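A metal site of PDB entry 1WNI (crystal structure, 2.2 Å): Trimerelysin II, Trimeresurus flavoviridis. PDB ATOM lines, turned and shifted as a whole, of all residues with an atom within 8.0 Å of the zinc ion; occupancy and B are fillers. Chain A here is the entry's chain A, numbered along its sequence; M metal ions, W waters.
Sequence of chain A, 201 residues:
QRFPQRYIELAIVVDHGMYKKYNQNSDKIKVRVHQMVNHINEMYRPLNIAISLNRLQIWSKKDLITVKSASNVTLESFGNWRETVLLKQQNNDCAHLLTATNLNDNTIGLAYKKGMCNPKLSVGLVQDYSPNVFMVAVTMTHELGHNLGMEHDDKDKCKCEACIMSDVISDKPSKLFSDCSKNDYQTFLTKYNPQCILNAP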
ATOM      1  N   GLY A 109       2.698 -10.244 -21.266  1.00  0.00           N
ATOM      2  CA  GLY A 109       3.572  -9.667 -20.280  1.00  0.00           C
ATOM      3  C   GLY A 109       3.631 -10.548 -19.049  1.00  0.00           C
ATOM      4  O   GLY A 109       2.655 -11.244 -18.742  1.00  0.00           O
ATOM      5  N   LEU A 110       4.752 -10.486 -18.340  1.00  0.00           N
ATOM      6  CA  LEU A 110       4.970 -11.241 -17.102  1.00  0.00           C
ATOM      7  C   LEU A 110       5.980 -10.472 -16.264  1.00  0.00           C
ATOM      8  O   LEU A 110       6.863  -9.818 -16.826  1.00  0.00           O
ATOM      9  CB  LEU A 110       5.555 -12.633 -17.430  1.00  0.00           C
ATOM     10  CG  LEU A 110       5.749 -13.642 -16.282  1.00  0.00           C
ATOM     11  CD1 LEU A 110       4.457 -13.994 -15.647  1.00  0.00           C
ATOM     12  CD2 LEU A 110       6.390 -14.884 -16.787  1.00  0.00           C
ATOM     13  N   ALA A 111       5.840 -10.510 -14.938  1.00  0.00           N
ATOM     14  CA  ALA A 111       6.767  -9.849 -14.009  1.00  0.00           C
ATOM     15  C   ALA A 111       6.719 -10.508 -12.639  1.00  0.00           C
ATOM     16  O   ALA A 111       5.715 -11.134 -12.300  1.00  0.00           O
ATOM     17  CB  ALA A 111       6.454  -8.367 -13.863  1.00  0.00           C
ATOM     18  N   LYS A 113       6.187 -10.440  -8.774  1.00  0.00           N
ATOM     19  CA  LYS A 113       5.419  -9.760  -7.739  1.00  0.00           C
ATOM     20  C   LYS A 113       6.373  -9.338  -6.614  1.00  0.00           C
ATOM     21  O   LYS A 113       7.246 -10.086  -6.215  1.00  0.00           O
ATOM     22  CB  LYS A 113       4.368 -10.715  -7.193  1.00  0.00           C
ATOM     23  CG  LYS A 113       3.117 -10.076  -6.620  1.00  0.00           C
ATOM     24  CD  LYS A 113       1.978 -10.053  -7.644  1.00  0.00           C
ATOM     25  CE  LYS A 113       1.414 -11.458  -7.941  1.00  0.00           C
ATOM     26  NZ  LYS A 113       0.161 -11.448  -8.803  1.00  0.00           N
ATOM     27  N   THR A 139       0.674  -2.285 -20.826  1.00  0.00           N
ATOM     28  CA  THR A 139       1.159  -3.603 -20.404  1.00  0.00           C
ATOM     29  C   THR A 139       2.435  -3.396 -19.601  1.00  0.00           C
ATOM     30  O   THR A 139       2.594  -3.976 -18.554  1.00  0.00           O
ATOM     31  CB  THR A 139       1.385  -4.575 -21.580  1.00  0.00           C
ATOM     32  OG1 THR A 139       0.166  -4.708 -22.309  1.00  0.00           O
ATOM     33  CG2 THR A 139       1.755  -5.952 -21.070  1.00  0.00           C
ATOM     34  N   HIS A 142       1.374  -2.060 -16.131  1.00  0.00           N
ATOM     35  CA  HIS A 142       0.736  -3.173 -15.411  1.00  0.00           C
ATOM     36  C   HIS A 142       1.797  -4.118 -14.778  1.00  0.00           C
ATOM     37  O   HIS A 142       1.720  -4.489 -13.587  1.00  0.00           O
ATOM     38  CB  HIS A 142      -0.136  -3.934 -16.408  1.00  0.00           C
ATOM     39  CG  HIS A 142      -0.854  -5.109 -15.815  1.00  0.00           C
ATOM     40  ND1 HIS A 142      -2.224  -5.228 -15.735  1.00  0.00           N
ATOM     41  CD2 HIS A 142      -0.359  -6.236 -15.237  1.00  0.00           C
ATOM     42  CE1 HIS A 142      -2.512  -6.374 -15.116  1.00  0.00           C
ATOM     43  NE2 HIS A 142      -1.411  -7.027 -14.800  1.00  0.00           N
ATOM     44  N   GLU A 143       2.785  -4.537 -15.583  1.00  0.00           N
ATOM     45  CA  GLU A 143       3.860  -5.397 -15.117  1.00  0.00           C
ATOM     46  C   GLU A 143       4.683  -4.704 -14.083  1.00  0.00           C
ATOM     47  O   GLU A 143       5.130  -5.338 -13.148  1.00  0.00           O
ATOM     48  CB  GLU A 143       4.749  -5.876 -16.262  1.00  0.00           C
ATOM     49  CG  GLU A 143       4.001  -6.763 -17.268  1.00  0.00           C
ATOM     50  CD  GLU A 143       3.121  -7.838 -16.603  1.00  0.00           C
ATOM     51  OE1 GLU A 143       2.120  -8.216 -17.222  1.00  0.00           O
ATOM     52  OE2 GLU A 143       3.415  -8.324 -15.480  1.00  0.00           O
ATOM     53  N   GLY A 145       3.521  -2.653 -12.146  1.00  0.00           N
ATOM     54  CA  GLY A 145       2.605  -2.697 -11.033  1.00  0.00           C
ATOM     55  C   GLY A 145       2.856  -3.935 -10.184  1.00  0.00           C
ATOM     56  O   GLY A 145       2.871  -3.829  -8.961  1.00  0.00           O
ATOM     57  N   HIS A 146       3.052  -5.100 -10.806  1.00  0.00           N
ATOM     58  CA  HIS A 146       3.370  -6.321 -10.029  1.00  0.00           C
ATOM     59  C   HIS A 146       4.733  -6.221  -9.294  1.00  0.00           C
ATOM     60  O   HIS A 146       4.849  -6.682  -8.157  1.00  0.00           O
ATOM     61  CB  HIS A 146       3.368  -7.567 -10.890  1.00  0.00           C
ATOM     62  CG  HIS A 146       2.013  -7.977 -11.346  1.00  0.00           C
ATOM     63  ND1 HIS A 146       0.923  -8.063 -10.522  1.00  0.00           N
ATOM     64  CD2 HIS A 146       1.570  -8.330 -12.580  1.00  0.00           C
ATOM     65  CE1 HIS A 146      -0.130  -8.474 -11.256  1.00  0.00           C
ATOM     66  NE2 HIS A 146       0.211  -8.643 -12.513  1.00  0.00           N
ATOM     67  N   MET A 150       1.468  -5.065  -6.620  1.00  0.00           N
ATOM     68  CA  MET A 150       0.056  -4.975  -6.985  1.00  0.00           C
ATOM     69  C   MET A 150      -0.514  -6.269  -7.521  1.00  0.00           C
ATOM     70  O   MET A 150       0.163  -6.983  -8.269  1.00  0.00           O
ATOM     71  CB  MET A 150      -0.167  -3.894  -8.032  1.00  0.00           C
ATOM     72  CG  MET A 150      -0.094  -2.500  -7.458  1.00  0.00           C
ATOM     73  SD  MET A 150      -0.160  -1.307  -8.771  1.00  0.00           S
ATOM     74  CE  MET A 150       0.731  -0.001  -8.155  1.00  0.00           C
ATOM     75  N   GLU A 151      -1.772  -6.568  -7.156  1.00  0.00           N
ATOM     76  CA  GLU A 151      -2.471  -7.769  -7.621  1.00  0.00           C
ATOM     77  C   GLU A 151      -3.473  -7.337  -8.678  1.00  0.00           C
ATOM     78  O   GLU A 151      -3.720  -6.152  -8.880  1.00  0.00           O
ATOM     79  CB  GLU A 151      -3.323  -8.418  -6.503  1.00  0.00           C
ATOM     80  CG  GLU A 151      -2.589  -9.001  -5.323  1.00  0.00           C
ATOM     81  CD  GLU A 151      -1.733 -10.181  -5.718  1.00  0.00           C
ATOM     82  OE1 GLU A 151      -2.285 -11.092  -6.385  1.00  0.00           O
ATOM     83  OE2 GLU A 151      -0.526 -10.176  -5.376  1.00  0.00           O
ATOM     84  N   HIS A 152      -4.110  -8.300  -9.310  1.00  0.00           N
ATOM     85  CA  HIS A 152      -5.129  -7.989 -10.279  1.00  0.00           C
ATOM     86  C   HIS A 152      -6.345  -7.421  -9.577  1.00  0.00           C
ATOM     87  O   HIS A 152      -6.454  -7.446  -8.353  1.00  0.00           O
ATOM     88  CB  HIS A 152      -5.521  -9.227 -11.034  1.00  0.00           C
ATOM     89  CG  HIS A 152      -4.467  -9.654 -11.983  1.00  0.00           C
ATOM     90  ND1 HIS A 152      -4.169 -10.962 -12.270  1.00  0.00           N
ATOM     91  CD2 HIS A 152      -3.593  -8.911 -12.692  1.00  0.00           C
ATOM     92  CE1 HIS A 152      -3.145 -10.955 -13.116  1.00  0.00           C
ATOM     93  NE2 HIS A 152      -2.766  -9.717 -13.391  1.00  0.00           N
ATOM     94  N   ASP A 153      -7.243  -6.855 -10.362  1.00  0.00           N
ATOM     95  CA  ASP A 153      -8.446  -6.264  -9.826  1.00  0.00           C
ATOM     96  C   ASP A 153      -9.557  -7.269  -9.828  1.00  0.00           C
ATOM     97  O   ASP A 153      -9.818  -7.914 -10.859  1.00  0.00           O
ATOM     98  CB  ASP A 153      -8.903  -5.071 -10.669  1.00  0.00           C
ATOM     99  CG  ASP A 153      -8.142  -3.798 -10.364  1.00  0.00           C
ATOM    100  OD1 ASP A 153      -7.639  -3.660  -9.226  1.00  0.00           O
ATOM    101  OD2 ASP A 153      -8.037  -2.940 -11.277  1.00  0.00           O
ATOM    102  N   ILE A 164      -5.760  -0.184 -14.835  1.00  0.00           N
ATOM    103  CA  ILE A 164      -4.480  -0.772 -15.198  1.00  0.00           C
ATOM    104  C   ILE A 164      -4.254  -2.214 -14.736  1.00  0.00           C
ATOM    105  O   ILE A 164      -3.733  -3.008 -15.510  1.00  0.00           O
ATOM    106  CB  ILE A 164      -3.338   0.144 -14.733  1.00  0.00           C
ATOM    107  CG1 ILE A 164      -3.295   1.380 -15.635  1.00  0.00           C
ATOM    108  CG2 ILE A 164      -2.006  -0.610 -14.752  1.00  0.00           C
ATOM    109  CD1 ILE A 164      -2.723   2.571 -14.991  1.00  0.00           C
ATOM    110  N   MET A 165      -4.701  -2.586 -13.538  1.00  0.00           N
ATOM    111  CA  MET A 165      -4.473  -3.942 -13.076  1.00  0.00           C
ATOM    112  C   MET A 165      -5.493  -5.049 -13.453  1.00  0.00           C
ATOM    113  O   MET A 165      -5.469  -6.130 -12.851  1.00  0.00           O
ATOM    114  CB  MET A 165      -4.134  -3.975 -11.587  1.00  0.00           C
ATOM    115  CG  MET A 165      -2.897  -3.195 -11.219  1.00  0.00           C
ATOM    116  SD  MET A 165      -1.349  -3.580 -12.096  1.00  0.00           S
ATOM    117  CE  MET A 165      -1.075  -5.294 -11.611  1.00  0.00           C
ATOM    118  N   SER A 166      -6.358  -4.810 -14.441  1.00  0.00           N
ATOM    119  CA  SER A 166      -7.291  -5.849 -14.873  1.00  0.00           C
ATOM    120  C   SER A 166      -6.442  -6.939 -15.509  1.00  0.00           C
ATOM    121  O   SER A 166      -5.478  -6.660 -16.210  1.00  0.00           O
ATOM    122  CB  SER A 166      -8.310  -5.328 -15.876  1.00  0.00           C
ATOM    123  OG  SER A 166      -7.695  -4.658 -16.939  1.00  0.00           O
ATOM    124  N   ASP A 167      -6.766  -8.184 -15.209  1.00  0.00           N
ATOM    125  CA  ASP A 167      -6.054  -9.348 -15.730  1.00  0.00           C
ATOM    126  C   ASP A 167      -5.992  -9.373 -17.251  1.00  0.00           C
ATOM    127  O   ASP A 167      -4.998  -9.807 -17.844  1.00  0.00           O
ATOM    128  CB  ASP A 167      -6.732 -10.608 -15.215  1.00  0.00           C
ATOM    129  CG  ASP A 167      -8.199 -10.383 -14.954  1.00  0.00           C
ATOM    130  OD1 ASP A 167      -8.589 -10.215 -13.780  1.00  0.00           O
ATOM    131  OD2 ASP A 167      -8.967 -10.311 -15.935  1.00  0.00           O
ATOM    132  N   VAL A 168      -7.078  -8.940 -17.886  1.00  0.00           N
ATOM    133  CA  VAL A 168      -7.105  -8.921 -19.338  1.00  0.00           C
ATOM    134  C   VAL A 168      -7.060  -7.471 -19.810  1.00  0.00           C
ATOM    135  O   VAL A 168      -7.816  -6.639 -19.317  1.00  0.00           O
ATOM    136  CB  VAL A 168      -8.377  -9.587 -19.862  1.00  0.00           C
ATOM    137  CG1 VAL A 168      -8.371  -9.630 -21.386  1.00  0.00           C
ATOM    138  CG2 VAL A 168      -8.498 -10.974 -19.298  1.00  0.00           C
HETATM  139 ZN    ZN M   1      -0.860  -9.316 -14.396  1.00  0.00          ZN
HETATM  140  O   HOH W   1      -0.323 -10.290 -16.564  1.00  0.00           O
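Of the 18 residues printed, 3 come within 4 Å of the zinc ion.
Along chain A the residues within 4 Å of the zinc ion span positions 142 to 152.
The nearest printed residue that does not touch the zinc ion is Glu 143 (4.3 Å).
A ring nitrogen (ND1) of His 142 is in hydrogen-bond range of the backbone carbonyl oxygen (O) of Ile 164.
ND1 of His 146 is in hydrogen-bond range of O of Met 150 (2.6 Å).
NE2 of His 152 is bound to the zinc ion (2.2 Å).
NE2 of His 146 is bound to the zinc ion, at 2.3 Å.
A ring nitrogen (NE2) of His 142 binds the zinc ion.
The zinc ion is bound by water W1, 2.4 Å away.
The zinc ion has four donor atoms within binding distance.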
